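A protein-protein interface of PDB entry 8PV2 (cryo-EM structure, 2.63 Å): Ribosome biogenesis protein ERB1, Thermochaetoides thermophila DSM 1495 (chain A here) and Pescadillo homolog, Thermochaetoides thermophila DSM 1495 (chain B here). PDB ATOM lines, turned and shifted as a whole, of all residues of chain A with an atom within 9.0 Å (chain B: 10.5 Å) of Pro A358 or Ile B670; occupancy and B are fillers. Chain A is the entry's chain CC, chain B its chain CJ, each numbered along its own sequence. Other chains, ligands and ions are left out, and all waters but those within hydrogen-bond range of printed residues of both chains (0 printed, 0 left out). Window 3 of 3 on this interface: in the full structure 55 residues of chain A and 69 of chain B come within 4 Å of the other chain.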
ATOM      1  N   TYR A 350      16.715 -27.221  -8.530  1.00  0.00           N
ATOM      2  CA  TYR A 350      16.232 -26.709  -7.251  1.00  0.00           C
ATOM      3  C   TYR A 350      15.051 -27.524  -6.747  1.00  0.00           C
ATOM      4  O   TYR A 350      14.739 -27.513  -5.551  1.00  0.00           O
ATOM      5  CB  TYR A 350      15.839 -25.239  -7.387  1.00  0.00           C
ATOM      6  CG  TYR A 350      16.969 -24.331  -7.804  1.00  0.00           C
ATOM      7  CD1 TYR A 350      18.146 -24.278  -7.073  1.00  0.00           C
ATOM      8  CD2 TYR A 350      16.856 -23.524  -8.926  1.00  0.00           C
ATOM      9  CE1 TYR A 350      19.181 -23.448  -7.450  1.00  0.00           C
ATOM     10  CE2 TYR A 350      17.885 -22.690  -9.310  1.00  0.00           C
ATOM     11  CZ  TYR A 350      19.045 -22.657  -8.569  1.00  0.00           C
ATOM     12  OH  TYR A 350      20.073 -21.828  -8.948  1.00  0.00           O
ATOM     13  N   SER A 353      15.689 -30.839  -4.150  1.00  0.00           N
ATOM     14  CA  SER A 353      16.083 -30.689  -2.753  1.00  0.00           C
ATOM     15  C   SER A 353      14.925 -31.007  -1.810  1.00  0.00           C
ATOM     16  O   SER A 353      13.750 -30.829  -2.143  1.00  0.00           O
ATOM     17  CB  SER A 353      16.593 -29.273  -2.492  1.00  0.00           C
ATOM     18  OG  SER A 353      15.610 -28.308  -2.810  1.00  0.00           O
ATOM     19  N   ASN A 355      14.313 -29.503   0.938  1.00  0.00           N
ATOM     20  CA  ASN A 355      13.784 -28.227   1.410  1.00  0.00           C
ATOM     21  C   ASN A 355      13.904 -27.226   0.267  1.00  0.00           C
ATOM     22  O   ASN A 355      14.809 -26.381   0.255  1.00  0.00           O
ATOM     23  CB  ASN A 355      14.525 -27.737   2.653  1.00  0.00           C
ATOM     24  CG  ASN A 355      13.808 -26.593   3.354  1.00  0.00           C
ATOM     25  OD1 ASN A 355      12.815 -26.061   2.857  1.00  0.00           O
ATOM     26  ND2 ASN A 355      14.313 -26.213   4.521  1.00  0.00           N
ATOM     27  N   PRO A 356      13.006 -27.296  -0.711  1.00  0.00           N
ATOM     28  CA  PRO A 356      13.097 -26.407  -1.860  1.00  0.00           C
ATOM     29  C   PRO A 356      12.453 -25.068  -1.556  1.00  0.00           C
ATOM     30  O   PRO A 356      11.800 -24.910  -0.513  1.00  0.00           O
ATOM     31  CB  PRO A 356      12.320 -27.168  -2.944  1.00  0.00           C
ATOM     32  CG  PRO A 356      11.291 -27.944  -2.181  1.00  0.00           C
ATOM     33  CD  PRO A 356      11.806 -28.150  -0.772  1.00  0.00           C
ATOM     34  N   PRO A 357      12.645 -24.071  -2.415  1.00  0.00           N
ATOM     35  CA  PRO A 357      11.819 -22.868  -2.347  1.00  0.00           C
ATOM     36  C   PRO A 357      10.354 -23.219  -2.535  1.00  0.00           C
ATOM     37  O   PRO A 357      10.024 -24.141  -3.295  1.00  0.00           O
ATOM     38  CB  PRO A 357      12.350 -22.016  -3.507  1.00  0.00           C
ATOM     39  CG  PRO A 357      13.775 -22.414  -3.611  1.00  0.00           C
ATOM     40  CD  PRO A 357      13.798 -23.888  -3.316  1.00  0.00           C
ATOM     41  N   PRO A 358       9.448 -22.517  -1.847  1.00  0.00           N
ATOM     42  CA  PRO A 358       8.053 -22.992  -1.778  1.00  0.00           C
ATOM     43  C   PRO A 358       7.288 -22.884  -3.086  1.00  0.00           C
ATOM     44  O   PRO A 358       6.200 -23.461  -3.205  1.00  0.00           O
ATOM     45  CB  PRO A 358       7.439 -22.097  -0.692  1.00  0.00           C
ATOM     46  CG  PRO A 358       8.289 -20.871  -0.691  1.00  0.00           C
ATOM     47  CD  PRO A 358       9.677 -21.336  -1.000  1.00  0.00           C
ATOM     48  N   GLU A 359       7.822 -22.166  -4.076  1.00  0.00           N
ATOM     49  CA  GLU A 359       7.099 -22.007  -5.332  1.00  0.00           C
ATOM     50  C   GLU A 359       7.174 -23.267  -6.186  1.00  0.00           C
ATOM     51  O   GLU A 359       6.455 -23.391  -7.184  1.00  0.00           O
ATOM     52  CB  GLU A 359       7.635 -20.803  -6.104  1.00  0.00           C
ATOM     53  CG  GLU A 359       9.051 -20.966  -6.607  1.00  0.00           C
ATOM     54  CD  GLU A 359      10.076 -20.432  -5.632  1.00  0.00           C
ATOM     55  OE1 GLU A 359       9.735 -20.240  -4.448  1.00  0.00           O
ATOM     56  OE2 GLU A 359      11.226 -20.193  -6.055  1.00  0.00           O
ATOM     57  N   TYR A 360       8.046 -24.208  -5.826  1.00  0.00           N
ATOM     58  CA  TYR A 360       8.124 -25.455  -6.579  1.00  0.00           C
ATOM     59  C   TYR A 360       7.083 -26.461  -6.107  1.00  0.00           C
ATOM     60  O   TYR A 360       6.800 -27.439  -6.807  1.00  0.00           O
ATOM     61  CB  TYR A 360       9.526 -26.048  -6.472  1.00  0.00           C
ATOM     62  CG  TYR A 360      10.577 -25.248  -7.192  1.00  0.00           C
ATOM     63  CD1 TYR A 360      10.572 -25.155  -8.575  1.00  0.00           C
ATOM     64  CD2 TYR A 360      11.573 -24.583  -6.493  1.00  0.00           C
ATOM     65  CE1 TYR A 360      11.529 -24.428  -9.244  1.00  0.00           C
ATOM     66  CE2 TYR A 360      12.536 -23.848  -7.153  1.00  0.00           C
ATOM     67  CZ  TYR A 360      12.509 -23.776  -8.529  1.00  0.00           C
ATOM     68  OH  TYR A 360      13.463 -23.050  -9.198  1.00  0.00           O
ATOM     69  N   LEU A 361       6.492 -26.230  -4.939  1.00  0.00           N
ATOM     70  CA  LEU A 361       5.602 -27.218  -4.346  1.00  0.00           C
ATOM     71  C   LEU A 361       4.296 -27.305  -5.133  1.00  0.00           C
ATOM     72  O   LEU A 361       3.772 -26.280  -5.583  1.00  0.00           O
ATOM     73  CB  LEU A 361       5.306 -26.876  -2.882  1.00  0.00           C
ATOM     74  CG  LEU A 361       6.251 -27.361  -1.775  1.00  0.00           C
ATOM     75  CD1 LEU A 361       6.274 -28.881  -1.728  1.00  0.00           C
ATOM     76  CD2 LEU A 361       7.665 -26.799  -1.898  1.00  0.00           C
ATOM     77  N   PRO A 362       3.753 -28.504  -5.327  1.00  0.00           N
ATOM     78  CA  PRO A 362       2.497 -28.630  -6.066  1.00  0.00           C
ATOM     79  C   PRO A 362       1.303 -28.602  -5.130  1.00  0.00           C
ATOM     80  O   PRO A 362       1.438 -28.550  -3.905  1.00  0.00           O
ATOM     81  CB  PRO A 362       2.632 -29.995  -6.741  1.00  0.00           C
ATOM     82  CG  PRO A 362       3.412 -30.793  -5.738  1.00  0.00           C
ATOM     83  CD  PRO A 362       4.307 -29.823  -4.980  1.00  0.00           C
ATOM     84  N   THR A 363       0.117 -28.636  -5.729  1.00  0.00           N
ATOM     85  CA  THR A 363      -1.105 -28.730  -4.949  1.00  0.00           C
ATOM     86  C   THR A 363      -1.415 -30.184  -4.609  1.00  0.00           C
ATOM     87  O   THR A 363      -0.878 -31.120  -5.213  1.00  0.00           O
ATOM     88  CB  THR A 363      -2.277 -28.113  -5.710  1.00  0.00           C
ATOM     89  N   PRO A 384       7.660 -32.690  -6.349  1.00  0.00           N
ATOM     90  CA  PRO A 384       8.256 -31.729  -5.414  1.00  0.00           C
ATOM     91  C   PRO A 384       7.789 -31.967  -3.986  1.00  0.00           C
ATOM     92  O   PRO A 384       6.631 -31.724  -3.642  1.00  0.00           O
ATOM     93  CB  PRO A 384       7.763 -30.379  -5.937  1.00  0.00           C
ATOM     94  CG  PRO A 384       7.475 -30.615  -7.378  1.00  0.00           C
ATOM     95  CD  PRO A 384       6.973 -32.019  -7.466  1.00  0.00           C
ATOM     96  N   LYS A 386       8.606 -31.440   0.245  1.00  0.00           N
ATOM     97  CA  LYS A 386       9.267 -30.659   1.280  1.00  0.00           C
ATOM     98  C   LYS A 386       9.177 -31.404   2.604  1.00  0.00           C
ATOM     99  O   LYS A 386       8.078 -31.740   3.056  1.00  0.00           O
ATOM    100  CB  LYS A 386       8.643 -29.268   1.417  1.00  0.00           C
ATOM    101  CG  LYS A 386       9.109 -28.511   2.651  1.00  0.00           C
ATOM    102  CD  LYS A 386       9.039 -27.007   2.443  1.00  0.00           C
ATOM    103  CE  LYS A 386       9.516 -26.253   3.674  1.00  0.00           C
ATOM    104  NZ  LYS A 386       9.600 -24.785   3.431  1.00  0.00           N
ATOM    105  N   GLN B 459      21.587 -28.773   7.755  1.00  0.00           N
ATOM    106  CA  GLN B 459      21.256 -27.942   6.603  1.00  0.00           C
ATOM    107  C   GLN B 459      22.143 -26.705   6.556  1.00  0.00           C
ATOM    108  O   GLN B 459      22.547 -26.264   5.472  1.00  0.00           O
ATOM    109  CB  GLN B 459      19.777 -27.554   6.638  1.00  0.00           C
ATOM    110  CG  GLN B 459      19.348 -26.632   5.506  1.00  0.00           C
ATOM    111  CD  GLN B 459      17.845 -26.536   5.369  1.00  0.00           C
ATOM    112  OE1 GLN B 459      17.101 -27.195   6.094  1.00  0.00           O
ATOM    113  NE2 GLN B 459      17.390 -25.715   4.430  1.00  0.00           N
ATOM    114  N   LEU B 482      14.339 -23.420   8.921  1.00  0.00           N
ATOM    115  CA  LEU B 482      15.543 -23.077   8.188  1.00  0.00           C
ATOM    116  C   LEU B 482      15.189 -22.474   6.829  1.00  0.00           C
ATOM    117  O   LEU B 482      14.098 -22.713   6.302  1.00  0.00           O
ATOM    118  CB  LEU B 482      16.418 -24.314   7.998  1.00  0.00           C
ATOM    119  N   PRO B 483      16.078 -21.664   6.259  1.00  0.00           N
ATOM    120  CA  PRO B 483      15.904 -21.213   4.872  1.00  0.00           C
ATOM    121  C   PRO B 483      15.913 -22.387   3.912  1.00  0.00           C
ATOM    122  O   PRO B 483      16.561 -23.411   4.183  1.00  0.00           O
ATOM    123  CB  PRO B 483      17.117 -20.299   4.644  1.00  0.00           C
ATOM    124  CG  PRO B 483      17.473 -19.810   5.992  1.00  0.00           C
ATOM    125  CD  PRO B 483      17.148 -20.921   6.948  1.00  0.00           C
ATOM    126  N   PRO B 484      15.184 -22.291   2.797  1.00  0.00           N
ATOM    127  CA  PRO B 484      15.128 -23.410   1.847  1.00  0.00           C
ATOM    128  C   PRO B 484      16.485 -23.690   1.217  1.00  0.00           C
ATOM    129  O   PRO B 484      17.246 -22.775   0.897  1.00  0.00           O
ATOM    130  CB  PRO B 484      14.111 -22.936   0.804  1.00  0.00           C
ATOM    131  CG  PRO B 484      14.120 -21.450   0.912  1.00  0.00           C
ATOM    132  CD  PRO B 484      14.359 -21.153   2.359  1.00  0.00           C
ATOM    133  N   HIS B 485      16.779 -24.975   1.041  1.00  0.00           N
ATOM    134  CA  HIS B 485      18.083 -25.381   0.544  1.00  0.00           C
ATOM    135  C   HIS B 485      18.151 -25.200  -0.969  1.00  0.00           C
ATOM    136  O   HIS B 485      17.150 -25.334  -1.678  1.00  0.00           O
ATOM    137  CB  HIS B 485      18.363 -26.834   0.927  1.00  0.00           C
ATOM    138  CG  HIS B 485      19.786 -27.248   0.727  1.00  0.00           C
ATOM    139  ND1 HIS B 485      20.265 -27.733  -0.471  1.00  0.00           N
ATOM    140  CD2 HIS B 485      20.839 -27.243   1.577  1.00  0.00           C
ATOM    141  CE1 HIS B 485      21.550 -28.010  -0.348  1.00  0.00           C
ATOM    142  NE2 HIS B 485      21.923 -27.721   0.884  1.00  0.00           N
ATOM    143  N   LEU B 486      19.349 -24.898  -1.464  1.00  0.00           N
ATOM    144  CA  LEU B 486      19.543 -24.569  -2.869  1.00  0.00           C
ATOM    145  C   LEU B 486      20.567 -25.504  -3.495  1.00  0.00           C
ATOM    146  O   LEU B 486      21.527 -25.936  -2.851  1.00  0.00           O
ATOM    147  CB  LEU B 486      19.992 -23.113  -3.046  1.00  0.00           C
ATOM    148  CG  LEU B 486      18.900 -22.050  -2.916  1.00  0.00           C
ATOM    149  CD1 LEU B 486      19.458 -20.681  -3.257  1.00  0.00           C
ATOM    150  CD2 LEU B 486      17.708 -22.382  -3.799  1.00  0.00           C
ATOM    151  N   TYR B 497      14.015 -19.459 -15.176  1.00  0.00           N
ATOM    152  CA  TYR B 497      13.586 -18.835 -13.922  1.00  0.00           C
ATOM    153  C   TYR B 497      14.594 -19.081 -12.801  1.00  0.00           C
ATOM    154  O   TYR B 497      15.216 -20.146 -12.728  1.00  0.00           O
ATOM    155  CB  TYR B 497      12.175 -19.297 -13.519  1.00  0.00           C
ATOM    156  CG  TYR B 497      11.845 -19.137 -12.053  1.00  0.00           C
ATOM    157  CD1 TYR B 497      11.492 -17.898 -11.541  1.00  0.00           C
ATOM    158  CD2 TYR B 497      11.867 -20.221 -11.187  1.00  0.00           C
ATOM    159  CE1 TYR B 497      11.188 -17.736 -10.208  1.00  0.00           C
ATOM    160  CE2 TYR B 497      11.563 -20.068  -9.847  1.00  0.00           C
ATOM    161  CZ  TYR B 497      11.223 -18.822  -9.366  1.00  0.00           C
ATOM    162  OH  TYR B 497      10.917 -18.653  -8.037  1.00  0.00           O
ATOM    163  N   PRO B 499      14.949 -18.796  -8.553  1.00  0.00           N
ATOM    164  CA  PRO B 499      14.377 -18.461  -7.235  1.00  0.00           C
ATOM    165  C   PRO B 499      15.110 -17.336  -6.527  1.00  0.00           C
ATOM    166  O   PRO B 499      14.489 -16.572  -5.779  1.00  0.00           O
ATOM    167  CB  PRO B 499      14.486 -19.774  -6.445  1.00  0.00           C
ATOM    168  CG  PRO B 499      15.035 -20.794  -7.367  1.00  0.00           C
ATOM    169  CD  PRO B 499      15.165 -20.238  -8.738  1.00  0.00           C
ATOM    170  N   THR B 500      16.423 -17.220  -6.735  1.00  0.00           N
ATOM    171  CA  THR B 500      17.185 -16.156  -6.091  1.00  0.00           C
ATOM    172  C   THR B 500      16.854 -14.798  -6.699  1.00  0.00           C
ATOM    173  O   THR B 500      16.956 -13.766  -6.027  1.00  0.00           O
ATOM    174  CB  THR B 500      18.683 -16.439  -6.204  1.00  0.00           C
ATOM    175  OG1 THR B 500      19.068 -16.435  -7.583  1.00  0.00           O
ATOM    176  CG2 THR B 500      19.009 -17.792  -5.603  1.00  0.00           C
ATOM    177  N   LEU B 503      11.111 -11.343  -7.950  1.00  0.00           N
ATOM    178  CA  LEU B 503       9.957 -11.357  -8.842  1.00  0.00           C
ATOM    179  C   LEU B 503       9.748  -9.991  -9.483  1.00  0.00           C
ATOM    180  O   LEU B 503       9.195  -9.889 -10.581  1.00  0.00           O
ATOM    181  CB  LEU B 503       8.714 -11.805  -8.069  1.00  0.00           C
ATOM    182  CG  LEU B 503       7.454 -12.224  -8.827  1.00  0.00           C
ATOM    183  CD1 LEU B 503       6.768 -13.362  -8.095  1.00  0.00           C
ATOM    184  CD2 LEU B 503       6.493 -11.055  -8.969  1.00  0.00           C
ATOM    185  N   LYS B 662       3.250 -20.314 -14.178  1.00  0.00           N
ATOM    186  CA  LYS B 662       2.658 -20.927 -12.990  1.00  0.00           C
ATOM    187  C   LYS B 662       3.578 -20.786 -11.782  1.00  0.00           C
ATOM    188  O   LYS B 662       3.125 -20.466 -10.669  1.00  0.00           O
ATOM    189  CB  LYS B 662       2.351 -22.397 -13.265  1.00  0.00           C
ATOM    190  CG  LYS B 662       1.695 -23.122 -12.109  1.00  0.00           C
ATOM    191  CD  LYS B 662       1.305 -24.533 -12.506  1.00  0.00           C
ATOM    192  CE  LYS B 662       2.530 -25.423 -12.623  1.00  0.00           C
ATOM    193  NZ  LYS B 662       2.165 -26.840 -12.896  1.00  0.00           N
ATOM    194  N   LEU B 663       4.882 -21.013 -11.991  1.00  0.00           N
ATOM    195  CA  LEU B 663       5.852 -20.835 -10.913  1.00  0.00           C
ATOM    196  C   LEU B 663       5.875 -19.393 -10.419  1.00  0.00           C
ATOM    197  O   LEU B 663       5.854 -19.147  -9.206  1.00  0.00           O
ATOM    198  CB  LEU B 663       7.245 -21.248 -11.386  1.00  0.00           C
ATOM    199  CG  LEU B 663       7.515 -22.735 -11.616  1.00  0.00           C
ATOM    200  CD1 LEU B 663       8.902 -22.931 -12.199  1.00  0.00           C
ATOM    201  CD2 LEU B 663       7.357 -23.520 -10.333  1.00  0.00           C
ATOM    202  N   ARG B 664       5.887 -18.430 -11.347  1.00  0.00           N
ATOM    203  CA  ARG B 664       5.905 -17.021 -10.961  1.00  0.00           C
ATOM    204  C   ARG B 664       4.622 -16.621 -10.243  1.00  0.00           C
ATOM    205  O   ARG B 664       4.660 -15.841  -9.284  1.00  0.00           O
ATOM    206  CB  ARG B 664       6.120 -16.140 -12.188  1.00  0.00           C
ATOM    207  CG  ARG B 664       7.513 -16.214 -12.779  1.00  0.00           C
ATOM    208  CD  ARG B 664       7.740 -15.060 -13.737  1.00  0.00           C
ATOM    209  NE  ARG B 664       6.704 -15.019 -14.761  1.00  0.00           N
ATOM    210  CZ  ARG B 664       6.833 -15.526 -15.978  1.00  0.00           C
ATOM    211  NH1 ARG B 664       7.961 -16.090 -16.375  1.00  0.00           N
ATOM    212  NH2 ARG B 664       5.805 -15.465 -16.818  1.00  0.00           N
ATOM    213  N   ALA B 665       3.478 -17.149 -10.685  1.00  0.00           N
ATOM    214  CA  ALA B 665       2.206 -16.800 -10.064  1.00  0.00           C
ATOM    215  C   ALA B 665       2.124 -17.309  -8.632  1.00  0.00           C
ATOM    216  O   ALA B 665       1.715 -16.573  -7.723  1.00  0.00           O
ATOM    217  CB  ALA B 665       1.049 -17.354 -10.893  1.00  0.00           C
ATOM    218  N   LYS B 666       2.524 -18.559  -8.392  1.00  0.00           N
ATOM    219  CA  LYS B 666       2.402 -19.045  -7.022  1.00  0.00           C
ATOM    220  C   LYS B 666       3.534 -18.511  -6.145  1.00  0.00           C
ATOM    221  O   LYS B 666       3.377 -18.406  -4.923  1.00  0.00           O
ATOM    222  CB  LYS B 666       2.307 -20.570  -6.992  1.00  0.00           C
ATOM    223  CG  LYS B 666       3.513 -21.351  -7.418  1.00  0.00           C
ATOM    224  CD  LYS B 666       3.326 -22.779  -6.930  1.00  0.00           C
ATOM    225  CE  LYS B 666       3.565 -22.885  -5.433  1.00  0.00           C
ATOM    226  NZ  LYS B 666       3.012 -24.142  -4.860  1.00  0.00           N
ATOM    227  N   ARG B 667       4.650 -18.082  -6.750  1.00  0.00           N
ATOM    228  CA  ARG B 667       5.633 -17.321  -5.983  1.00  0.00           C
ATOM    229  C   ARG B 667       5.089 -15.955  -5.587  1.00  0.00           C
ATOM    230  O   ARG B 667       5.393 -15.451  -4.499  1.00  0.00           O
ATOM    231  CB  ARG B 667       6.933 -17.153  -6.765  1.00  0.00           C
ATOM    232  CG  ARG B 667       8.108 -16.813  -5.863  1.00  0.00           C
ATOM    233  CD  ARG B 667       9.226 -16.106  -6.607  1.00  0.00           C
ATOM    234  NE  ARG B 667      10.443 -16.044  -5.806  1.00  0.00           N
ATOM    235  CZ  ARG B 667      11.387 -15.125  -5.946  1.00  0.00           C
ATOM    236  NH1 ARG B 667      11.304 -14.183  -6.870  1.00  0.00           N
ATOM    237  NH2 ARG B 667      12.441 -15.150  -5.136  1.00  0.00           N
ATOM    238  N   ARG B 668       4.297 -15.332  -6.464  1.00  0.00           N
ATOM    239  CA  ARG B 668       3.618 -14.091  -6.099  1.00  0.00           C
ATOM    240  C   ARG B 668       2.635 -14.326  -4.961  1.00  0.00           C
ATOM    241  O   ARG B 668       2.477 -13.474  -4.079  1.00  0.00           O
ATOM    242  CB  ARG B 668       2.896 -13.508  -7.312  1.00  0.00           C
ATOM    243  CG  ARG B 668       2.320 -12.119  -7.086  1.00  0.00           C
ATOM    244  CD  ARG B 668       1.428 -11.679  -8.239  1.00  0.00           C
ATOM    245  NE  ARG B 668       1.785 -12.316  -9.501  1.00  0.00           N
ATOM    246  CZ  ARG B 668       2.683 -11.843 -10.354  1.00  0.00           C
ATOM    247  NH1 ARG B 668       3.329 -10.712 -10.119  1.00  0.00           N
ATOM    248  NH2 ARG B 668       2.937 -12.519 -11.470  1.00  0.00           N
ATOM    249  N   ARG B 669       1.965 -15.482  -4.970  1.00  0.00           N
ATOM    250  CA  ARG B 669       1.101 -15.847  -3.849  1.00  0.00           C
ATOM    251  C   ARG B 669       1.885 -15.972  -2.546  1.00  0.00           C
ATOM    252  O   ARG B 669       1.444 -15.476  -1.501  1.00  0.00           O
ATOM    253  CB  ARG B 669       0.365 -17.152  -4.152  1.00  0.00           C
ATOM    254  CG  ARG B 669      -0.588 -17.063  -5.321  1.00  0.00           C
ATOM    255  CD  ARG B 669      -1.774 -16.184  -4.974  1.00  0.00           C
ATOM    256  NE  ARG B 669      -2.769 -16.166  -6.038  1.00  0.00           N
ATOM    257  CZ  ARG B 669      -2.788 -15.286  -7.029  1.00  0.00           C
ATOM    258  NH1 ARG B 669      -1.875 -14.333  -7.123  1.00  0.00           N
ATOM    259  NH2 ARG B 669      -3.746 -15.364  -7.948  1.00  0.00           N
ATOM    260  N   ILE B 670       3.050 -16.628  -2.588  1.00  0.00           N
ATOM    261  CA  ILE B 670       3.885 -16.756  -1.390  1.00  0.00           C
ATOM    262  C   ILE B 670       4.362 -15.387  -0.913  1.00  0.00           C
ATOM    263  O   ILE B 670       4.397 -15.112   0.294  1.00  0.00           O
ATOM    264  CB  ILE B 670       5.068 -17.711  -1.651  1.00  0.00           C
ATOM    265  CG1 ILE B 670       4.567 -19.097  -2.053  1.00  0.00           C
ATOM    266  CG2 ILE B 670       5.964 -17.828  -0.427  1.00  0.00           C
ATOM    267  CD1 ILE B 670       3.723 -19.771  -0.996  1.00  0.00           C
ATOM    268  N   GLU B 671       4.724 -14.506  -1.851  1.00  0.00           N
ATOM    269  CA  GLU B 671       5.132 -13.150  -1.492  1.00  0.00           C
ATOM    270  C   GLU B 671       3.989 -12.373  -0.848  1.00  0.00           C
ATOM    271  O   GLU B 671       4.209 -11.591   0.084  1.00  0.00           O
ATOM    272  CB  GLU B 671       5.643 -12.410  -2.729  1.00  0.00           C
ATOM    273  CG  GLU B 671       6.987 -12.893  -3.240  1.00  0.00           C
ATOM    274  CD  GLU B 671       8.126 -12.539  -2.310  1.00  0.00           C
ATOM    275  OE1 GLU B 671       8.062 -11.468  -1.670  1.00  0.00           O
ATOM    276  OE2 GLU B 671       9.088 -13.329  -2.220  1.00  0.00           O
ATOM    277  N   LYS B 672       2.764 -12.570  -1.339  1.00  0.00           N
ATOM    278  CA  LYS B 672       1.612 -11.895  -0.749  1.00  0.00           C
ATOM    279  C   LYS B 672       1.316 -12.439   0.643  1.00  0.00           C
ATOM    280  O   LYS B 672       0.882 -11.694   1.530  1.00  0.00           O
ATOM    281  CB  LYS B 672       0.402 -12.033  -1.683  1.00  0.00           C
ATOM    282  CG  LYS B 672      -0.905 -11.358  -1.234  1.00  0.00           C
ATOM    283  CD  LYS B 672      -1.847 -12.291  -0.471  1.00  0.00           C
ATOM    284  CE  LYS B 672      -2.451 -13.340  -1.389  1.00  0.00           C
ATOM    285  NZ  LYS B 672      -3.378 -14.245  -0.656  1.00  0.00           N
ATOM    286  N   GLU B 673       1.543 -13.733   0.857  1.00  0.00           N
ATOM    287  CA  GLU B 673       1.348 -14.322   2.180  1.00  0.00           C
ATOM    288  C   GLU B 673       2.421 -13.853   3.160  1.00  0.00           C
ATOM    289  O   GLU B 673       3.466 -13.342   2.757  1.00  0.00           O
ATOM    290  CB  GLU B 673       1.351 -15.849   2.101  1.00  0.00           C
ATOM    291  CG  GLU B 673       0.194 -16.440   1.315  1.00  0.00           C
ATOM    292  CD  GLU B 673       0.549 -17.768   0.675  1.00  0.00           C
ATOM    293  OE1 GLU B 673       1.505 -18.418   1.147  1.00  0.00           O
ATOM    294  OE2 GLU B 673      -0.123 -18.158  -0.303  1.00  0.00           O
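The side-chain amide nitrogen of Gln B459 lies close to the side-chain amide nitrogen of Asn A355 (3.1 Å).
The backbone carbonyl oxygen of Asn A355 is in hydrogen-bond range of the backbone NH of His B485 (2.5 Å).
The side-chain hydroxyl (OH) of Tyr B497 sits at hydrogen-bond distance from the side-chain carboxylate (OE2) of Glu A359, 2.5 Å away.
O of Leu A361 sits close to NZ of Lys B666, 2.4 Å away.
O of Tyr A350 sits at hydrogen-bond distance from OG of Ser A353, at 3.0 Å.
The side-chain amide nitrogen of Gln B459 lies within hydrogen-bond range of the backbone carbonyl oxygen of Pro B483 (2.5 Å).
The side-chain hydroxyl (OH) of Tyr B497 lies close to the guanidinium group (NE) of Arg B667, at 3.5 Å.
The backbone carbonyl oxygen (O) of Pro B499 sits at hydrogen-bond distance from the guanidinium group (NH2) of Arg B667.
OG of Ser A353 touches O of His B485, 3.5 Å away.
O of Leu B482 touches ND2 of Asn A355 (3.9 Å).
O of Pro B483 touches ND2 of Asn A355, at 3.6 Å.
O of Pro A356 touches CB of Pro B484, 3.3 Å away.
N of Pro A357 touches CB of Pro B484, 3.7 Å away.
CD2 of Leu B486 touches CG of Pro A357 (3.9 Å).
Pro A357 touches Pro B499.
Glu A359 touches Lys B666 (O to CD, 3.2 Å).
OH of Tyr A360 touches CE2 of Tyr B497 (3.6 Å).
Pro B499 touches Tyr A360.
Pro A358 touches just these residues of chain B: Lys B666 (3.5 Å) and Ile B670 (3.8 Å).
Ile B670 touches one residue of chain A.
Pro A356 touches just one residue of chain B: Pro B484.
Glu A359 touches just these residues of chain B: Tyr B497, Pro B499, Leu B663, Lys B666 and Arg B667.
Printed residues of chain B within 4 Å of Leu A361: Lys B666 (2.4 Å).
No residue of chain A comes within 4 Å of Glu B673.
Of the printed residues of chain B, Pro A357 touches Pro B484 (3.7 Å), Leu B486 (3.9 Å) and Pro B499 (3.9 Å).
Of the printed residues of chain A, Pro B483 touches Asn A355.
Printed residues of chain A within 4 Å of Leu B482: Asn A355.
Ala B665 touches none of the printed residues of chain A.
Leu B503 touches none of the printed residues of chain A.
The nearest residue of chain A that does not touch Ile B670 is Glu A359 (4.9 Å).
Of the 13 printed residues of chain A, 9 touch a printed residue of chain B.
Hydrophobic or aromatic side chains of chain B that line the printed part of chain A: Pro B484, His B485, Leu B486, Tyr B497, Pro B499, Leu B663 and Ile B670.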
